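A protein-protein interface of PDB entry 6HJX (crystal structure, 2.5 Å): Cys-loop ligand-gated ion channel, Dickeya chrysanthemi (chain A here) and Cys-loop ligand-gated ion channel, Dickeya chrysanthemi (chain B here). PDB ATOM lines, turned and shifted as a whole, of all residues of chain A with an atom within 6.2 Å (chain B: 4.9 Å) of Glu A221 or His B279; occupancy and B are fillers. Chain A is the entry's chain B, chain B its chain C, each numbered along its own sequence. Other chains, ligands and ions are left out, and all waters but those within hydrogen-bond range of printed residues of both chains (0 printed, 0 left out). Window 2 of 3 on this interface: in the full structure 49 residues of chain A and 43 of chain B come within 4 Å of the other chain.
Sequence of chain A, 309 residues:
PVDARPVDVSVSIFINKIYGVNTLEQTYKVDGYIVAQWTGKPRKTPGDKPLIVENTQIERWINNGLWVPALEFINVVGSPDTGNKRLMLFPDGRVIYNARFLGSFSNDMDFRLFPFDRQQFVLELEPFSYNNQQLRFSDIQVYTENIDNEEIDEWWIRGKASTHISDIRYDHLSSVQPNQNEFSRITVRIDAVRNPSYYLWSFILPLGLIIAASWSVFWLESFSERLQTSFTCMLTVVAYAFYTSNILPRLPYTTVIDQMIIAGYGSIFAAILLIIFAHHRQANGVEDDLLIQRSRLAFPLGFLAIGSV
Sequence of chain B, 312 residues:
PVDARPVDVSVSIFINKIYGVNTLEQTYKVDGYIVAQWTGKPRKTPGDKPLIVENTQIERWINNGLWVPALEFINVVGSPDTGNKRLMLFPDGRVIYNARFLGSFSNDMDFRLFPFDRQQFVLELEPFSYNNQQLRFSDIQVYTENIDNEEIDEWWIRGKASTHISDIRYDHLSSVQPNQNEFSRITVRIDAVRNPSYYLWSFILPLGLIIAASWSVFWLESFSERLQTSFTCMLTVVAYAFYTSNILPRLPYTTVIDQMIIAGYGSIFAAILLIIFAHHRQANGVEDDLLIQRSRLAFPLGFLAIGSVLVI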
ATOM      1  N   VAL A 217       5.385 -19.182 -23.105  1.00  0.00           N
ATOM      2  CA  VAL A 217       6.702 -18.599 -23.337  1.00  0.00           C
ATOM      3  C   VAL A 217       7.798 -19.526 -22.832  1.00  0.00           C
ATOM      4  O   VAL A 217       8.908 -19.541 -23.376  1.00  0.00           O
ATOM      5  CB  VAL A 217       6.801 -17.206 -22.680  1.00  0.00           C
ATOM      6  CG1 VAL A 217       5.806 -16.251 -23.311  1.00  0.00           C
ATOM      7  CG2 VAL A 217       6.585 -17.299 -21.170  1.00  0.00           C
ATOM      8  N   TRP A 219       7.997 -22.580 -23.230  1.00  0.00           N
ATOM      9  CA  TRP A 219       8.229 -23.628 -24.211  1.00  0.00           C
ATOM     10  C   TRP A 219       9.026 -23.141 -25.414  1.00  0.00           C
ATOM     11  O   TRP A 219       9.364 -23.953 -26.283  1.00  0.00           O
ATOM     12  CB  TRP A 219       6.893 -24.210 -24.684  1.00  0.00           C
ATOM     13  CG  TRP A 219       6.088 -24.794 -23.571  1.00  0.00           C
ATOM     14  CD1 TRP A 219       5.301 -24.117 -22.690  1.00  0.00           C
ATOM     15  CD2 TRP A 219       5.995 -26.176 -23.211  1.00  0.00           C
ATOM     16  NE1 TRP A 219       4.720 -24.989 -21.805  1.00  0.00           N
ATOM     17  CE2 TRP A 219       5.129 -26.262 -22.105  1.00  0.00           C
ATOM     18  CE3 TRP A 219       6.559 -27.350 -23.719  1.00  0.00           C
ATOM     19  CZ2 TRP A 219       4.813 -27.473 -21.497  1.00  0.00           C
ATOM     20  CZ3 TRP A 219       6.243 -28.551 -23.115  1.00  0.00           C
ATOM     21  CH2 TRP A 219       5.378 -28.604 -22.015  1.00  0.00           C
ATOM     22  N   LEU A 220       9.320 -21.847 -25.492  1.00  0.00           N
ATOM     23  CA  LEU A 220      10.210 -21.340 -26.524  1.00  0.00           C
ATOM     24  C   LEU A 220      11.650 -21.713 -26.194  1.00  0.00           C
ATOM     25  O   LEU A 220      12.016 -21.916 -25.033  1.00  0.00           O
ATOM     26  CB  LEU A 220      10.066 -19.826 -26.657  1.00  0.00           C
ATOM     27  CG  LEU A 220       8.701 -19.352 -27.156  1.00  0.00           C
ATOM     28  CD1 LEU A 220       8.449 -17.913 -26.731  1.00  0.00           C
ATOM     29  CD2 LEU A 220       8.611 -19.487 -28.667  1.00  0.00           C
ATOM     30  N   GLU A 221      12.476 -21.794 -27.234  1.00  0.00           N
ATOM     31  CA  GLU A 221      13.785 -22.423 -27.110  1.00  0.00           C
ATOM     32  C   GLU A 221      14.896 -21.459 -26.718  1.00  0.00           C
ATOM     33  O   GLU A 221      15.818 -21.858 -25.995  1.00  0.00           O
ATOM     34  CB  GLU A 221      14.136 -23.118 -28.426  1.00  0.00           C
ATOM     35  CG  GLU A 221      13.255 -24.324 -28.703  1.00  0.00           C
ATOM     36  CD  GLU A 221      13.269 -24.747 -30.157  1.00  0.00           C
ATOM     37  OE1 GLU A 221      13.655 -23.929 -31.019  1.00  0.00           O
ATOM     38  OE2 GLU A 221      12.887 -25.901 -30.438  1.00  0.00           O
ATOM     39  N   SER A 222      14.840 -20.208 -27.162  1.00  0.00           N
ATOM     40  CA  SER A 222      15.880 -19.234 -26.870  1.00  0.00           C
ATOM     41  C   SER A 222      15.381 -18.191 -25.877  1.00  0.00           C
ATOM     42  O   SER A 222      14.202 -17.828 -25.867  1.00  0.00           O
ATOM     43  CB  SER A 222      16.353 -18.534 -28.147  1.00  0.00           C
ATOM     44  OG  SER A 222      15.376 -17.624 -28.617  1.00  0.00           O
ATOM     45  N   PHE A 223      16.304 -17.712 -25.039  1.00  0.00           N
ATOM     46  CA  PHE A 223      15.988 -16.638 -24.103  1.00  0.00           C
ATOM     47  C   PHE A 223      15.415 -15.429 -24.833  1.00  0.00           C
ATOM     48  O   PHE A 223      14.405 -14.853 -24.410  1.00  0.00           O
ATOM     49  CB  PHE A 223      17.249 -16.260 -23.321  1.00  0.00           C
ATOM     50  CG  PHE A 223      17.217 -14.875 -22.737  1.00  0.00           C
ATOM     51  CD1 PHE A 223      16.575 -14.627 -21.535  1.00  0.00           C
ATOM     52  CD2 PHE A 223      17.847 -13.824 -23.385  1.00  0.00           C
ATOM     53  CE1 PHE A 223      16.554 -13.353 -20.996  1.00  0.00           C
ATOM     54  CE2 PHE A 223      17.829 -12.551 -22.850  1.00  0.00           C
ATOM     55  CZ  PHE A 223      17.182 -12.314 -21.654  1.00  0.00           C
ATOM     56  N   GLU A 225      13.713 -15.310 -27.441  1.00  0.00           N
ATOM     57  CA  GLU A 225      12.337 -15.560 -27.858  1.00  0.00           C
ATOM     58  C   GLU A 225      11.374 -15.460 -26.681  1.00  0.00           C
ATOM     59  O   GLU A 225      10.258 -14.947 -26.826  1.00  0.00           O
ATOM     60  CB  GLU A 225      12.229 -16.937 -28.513  1.00  0.00           C
ATOM     61  CG  GLU A 225      12.768 -16.994 -29.931  1.00  0.00           C
ATOM     62  CD  GLU A 225      12.854 -18.413 -30.462  1.00  0.00           C
ATOM     63  OE1 GLU A 225      13.133 -19.335 -29.667  1.00  0.00           O
ATOM     64  OE2 GLU A 225      12.639 -18.606 -31.675  1.00  0.00           O
ATOM     65  N   ARG A 226      11.785 -15.950 -25.509  1.00  0.00           N
ATOM     66  CA  ARG A 226      10.901 -15.931 -24.351  1.00  0.00           C
ATOM     67  C   ARG A 226      10.632 -14.512 -23.872  1.00  0.00           C
ATOM     68  O   ARG A 226       9.534 -14.222 -23.381  1.00  0.00           O
ATOM     69  CB  ARG A 226      11.502 -16.772 -23.223  1.00  0.00           C
ATOM     70  CG  ARG A 226      11.697 -18.232 -23.604  1.00  0.00           C
ATOM     71  CD  ARG A 226      12.053 -19.110 -22.416  1.00  0.00           C
ATOM     72  NE  ARG A 226      13.451 -18.965 -22.017  1.00  0.00           N
ATOM     73  CZ  ARG A 226      14.475 -19.546 -22.638  1.00  0.00           C
ATOM     74  NH1 ARG A 226      14.270 -20.310 -23.705  1.00  0.00           N
ATOM     75  NH2 ARG A 226      15.710 -19.355 -22.197  1.00  0.00           N
ATOM     76  N   ARG A 296       7.472 -25.079 -16.885  1.00  0.00           N
ATOM     77  CA  ARG A 296       6.294 -24.936 -17.712  1.00  0.00           C
ATOM     78  C   ARG A 296       5.106 -25.517 -16.995  1.00  0.00           C
ATOM     79  O   ARG A 296       3.965 -25.165 -17.301  1.00  0.00           O
ATOM     80  CB  ARG A 296       6.530 -25.633 -19.045  1.00  0.00           C
ATOM     81  CG  ARG A 296       7.834 -25.214 -19.724  1.00  0.00           C
ATOM     82  CD  ARG A 296       8.553 -26.379 -20.374  1.00  0.00           C
ATOM     83  NE  ARG A 296       9.460 -25.912 -21.413  1.00  0.00           N
ATOM     84  CZ  ARG A 296      10.164 -26.706 -22.210  1.00  0.00           C
ATOM     85  NH1 ARG A 296      10.073 -28.020 -22.093  1.00  0.00           N
ATOM     86  NH2 ARG A 296      10.962 -26.177 -23.128  1.00  0.00           N
ATOM     87  N   PHE B 223       8.787 -24.041 -35.461  1.00  0.00           N
ATOM     88  CA  PHE B 223       8.001 -23.950 -34.233  1.00  0.00           C
ATOM     89  C   PHE B 223       7.978 -22.523 -33.701  1.00  0.00           C
ATOM     90  O   PHE B 223       6.920 -22.000 -33.331  1.00  0.00           O
ATOM     91  CB  PHE B 223       8.564 -24.906 -33.180  1.00  0.00           C
ATOM     92  CG  PHE B 223       8.046 -24.652 -31.792  1.00  0.00           C
ATOM     93  CD1 PHE B 223       6.820 -25.155 -31.393  1.00  0.00           C
ATOM     94  CD2 PHE B 223       8.789 -23.911 -30.887  1.00  0.00           C
ATOM     95  CE1 PHE B 223       6.342 -24.923 -30.116  1.00  0.00           C
ATOM     96  CE2 PHE B 223       8.316 -23.677 -29.610  1.00  0.00           C
ATOM     97  CZ  PHE B 223       7.092 -24.184 -29.224  1.00  0.00           C
ATOM     98  N   ILE B 275       0.507 -26.650 -31.578  1.00  0.00           N
ATOM     99  CA  ILE B 275       1.863 -26.293 -31.989  1.00  0.00           C
ATOM    100  C   ILE B 275       2.879 -26.780 -30.963  1.00  0.00           C
ATOM    101  O   ILE B 275       3.963 -27.261 -31.321  1.00  0.00           O
ATOM    102  CB  ILE B 275       1.961 -24.772 -32.214  1.00  0.00           C
ATOM    103  CG1 ILE B 275       1.175 -24.377 -33.465  1.00  0.00           C
ATOM    104  CG2 ILE B 275       3.414 -24.329 -32.336  1.00  0.00           C
ATOM    105  CD1 ILE B 275       0.924 -22.894 -33.586  1.00  0.00           C
ATOM    106  N   ILE B 276       2.551 -26.667 -29.676  1.00  0.00           N
ATOM    107  CA  ILE B 276       3.487 -27.082 -28.636  1.00  0.00           C
ATOM    108  C   ILE B 276       3.529 -28.598 -28.527  1.00  0.00           C
ATOM    109  O   ILE B 276       4.600 -29.190 -28.358  1.00  0.00           O
ATOM    110  CB  ILE B 276       3.113 -26.423 -27.295  1.00  0.00           C
ATOM    111  CG1 ILE B 276       3.431 -24.929 -27.356  1.00  0.00           C
ATOM    112  CG2 ILE B 276       3.852 -27.086 -26.134  1.00  0.00           C
ATOM    113  CD1 ILE B 276       2.967 -24.146 -26.153  1.00  0.00           C
ATOM    114  N   PHE B 277       2.370 -29.251 -28.617  1.00  0.00           N
ATOM    115  CA  PHE B 277       2.333 -30.702 -28.492  1.00  0.00           C
ATOM    116  C   PHE B 277       3.150 -31.362 -29.597  1.00  0.00           C
ATOM    117  O   PHE B 277       3.987 -32.233 -29.331  1.00  0.00           O
ATOM    118  CB  PHE B 277       0.888 -31.197 -28.521  1.00  0.00           C
ATOM    119  CG  PHE B 277       0.764 -32.693 -28.498  1.00  0.00           C
ATOM    120  CD1 PHE B 277       0.791 -33.386 -27.299  1.00  0.00           C
ATOM    121  CD2 PHE B 277       0.631 -33.408 -29.677  1.00  0.00           C
ATOM    122  CE1 PHE B 277       0.683 -34.763 -27.275  1.00  0.00           C
ATOM    123  CE2 PHE B 277       0.521 -34.784 -29.660  1.00  0.00           C
ATOM    124  CZ  PHE B 277       0.548 -35.463 -28.458  1.00  0.00           C
ATOM    125  N   ALA B 278       2.923 -30.953 -30.846  1.00  0.00           N
ATOM    126  CA  ALA B 278       3.657 -31.528 -31.966  1.00  0.00           C
ATOM    127  C   ALA B 278       5.162 -31.424 -31.759  1.00  0.00           C
ATOM    128  O   ALA B 278       5.905 -32.372 -32.042  1.00  0.00           O
ATOM    129  CB  ALA B 278       3.251 -30.828 -33.263  1.00  0.00           C
ATOM    130  N   HIS B 279       5.629 -30.282 -31.255  1.00  0.00           N
ATOM    131  CA  HIS B 279       7.062 -30.021 -31.184  1.00  0.00           C
ATOM    132  C   HIS B 279       7.709 -30.620 -29.941  1.00  0.00           C
ATOM    133  O   HIS B 279       8.900 -30.948 -29.971  1.00  0.00           O
ATOM    134  CB  HIS B 279       7.312 -28.512 -31.220  1.00  0.00           C
ATOM    135  CG  HIS B 279       8.752 -28.135 -31.079  1.00  0.00           C
ATOM    136  ND1 HIS B 279       9.356 -27.943 -29.854  1.00  0.00           N
ATOM    137  CD2 HIS B 279       9.711 -27.912 -32.009  1.00  0.00           C
ATOM    138  CE1 HIS B 279      10.624 -27.620 -30.035  1.00  0.00           C
ATOM    139  NE2 HIS B 279      10.865 -27.594 -31.334  1.00  0.00           N
ATOM    140  N   HIS B 280       6.958 -30.772 -28.851  1.00  0.00           N
ATOM    141  CA  HIS B 280       7.512 -31.230 -27.583  1.00  0.00           C
ATOM    142  C   HIS B 280       7.048 -32.629 -27.199  1.00  0.00           C
ATOM    143  O   HIS B 280       7.331 -33.079 -26.084  1.00  0.00           O
ATOM    144  CB  HIS B 280       7.166 -30.238 -26.470  1.00  0.00           C
ATOM    145  CG  HIS B 280       7.989 -28.989 -26.500  1.00  0.00           C
ATOM    146  ND1 HIS B 280       9.227 -28.901 -25.900  1.00  0.00           N
ATOM    147  CD2 HIS B 280       7.757 -27.779 -27.063  1.00  0.00           C
ATOM    148  CE1 HIS B 280       9.720 -27.689 -26.089  1.00  0.00           C
ATOM    149  NE2 HIS B 280       8.848 -26.989 -26.792  1.00  0.00           N
ATOM    150  N   ARG B 281       6.345 -33.326 -28.091  1.00  0.00           N
ATOM    151  CA  ARG B 281       5.985 -34.718 -27.850  1.00  0.00           C
ATOM    152  C   ARG B 281       7.019 -35.690 -28.401  1.00  0.00           C
ATOM    153  O   ARG B 281       7.225 -36.760 -27.817  1.00  0.00           O
ATOM    154  CB  ARG B 281       4.618 -35.025 -28.469  1.00  0.00           C
ATOM    155  N   GLN B 282       7.676 -35.336 -29.501  1.00  0.00           N
ATOM    156  CA  GLN B 282       8.664 -36.200 -30.133  1.00  0.00           C
ATOM    157  C   GLN B 282       9.923 -35.375 -30.394  1.00  0.00           C
ATOM    158  O   GLN B 282      10.157 -34.325 -29.782  1.00  0.00           O
ATOM    159  CB  GLN B 282       8.092 -36.817 -31.416  1.00  0.00           C
ATOM    160  N   ASP B 289       7.586 -33.826 -36.030  1.00  0.00           N
ATOM    161  CA  ASP B 289       6.841 -32.625 -35.667  1.00  0.00           C
ATOM    162  C   ASP B 289       6.209 -31.979 -36.896  1.00  0.00           C
ATOM    163  O   ASP B 289       5.004 -31.707 -36.920  1.00  0.00           O
ATOM    164  CB  ASP B 289       7.767 -31.641 -34.952  1.00  0.00           C
ATOM    165  CG  ASP B 289       7.163 -30.255 -34.828  1.00  0.00           C
ATOM    166  OD1 ASP B 289       6.093 -30.123 -34.197  1.00  0.00           O
ATOM    167  OD2 ASP B 289       7.760 -29.296 -35.361  1.00  0.00           O
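O of Trp A219 is in hydrogen-bond range of NE2 of His B280 (3.1 Å). The side-chain carboxylate (OE2) of Glu A221 lies within hydrogen-bond range of a ring nitrogen (NE2) of His B279.
The backbone NH of His B279 sits at hydrogen-bond distance from the side-chain carboxylate of Asp B289 (3.0 Å). O of Glu A221 sits at hydrogen-bond distance from NH1 of Arg A226 (3.2 Å). ND1 of His B279 sits close to NE2 of His B280 (3.2 Å).
Among the printed residues, pairs that only touch across the chains: Trp A219 with Phe B223 (3.5 Å), Arg A296 with His B280 (3.5 Å) and Trp A219 with Ile B276 (3.6 Å).
Printed residues of chain B within 4 Å of Glu A221: His B279. His B279 touches one residue of chain A. Printed residues of chain B within 4 Å of Trp A219: Phe B223, Ile B276 and His B280. Of the printed residues of chain A, Ile B276 touches Trp A219. Printed residues of chain A within 4 Å of Phe B223: Trp A219 (3.5 Å). Printed residues of chain B within 4 Å of Arg A296: His B280. The nearest residue of chain B that does not touch Glu A221 is Phe B223 (4.6 Å). The nearest residue of chain A that does not touch His B279 is Trp A219 (5.4 Å). The nearest printed residue of chain B that does not touch Arg A296 is His B279 (7.1 Å).
Of the 9 printed residues of chain A, 3 touch a printed residue of chain B. Hydrophobic or aromatic side chains of chain A that line the printed part of chain B: Trp A219.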
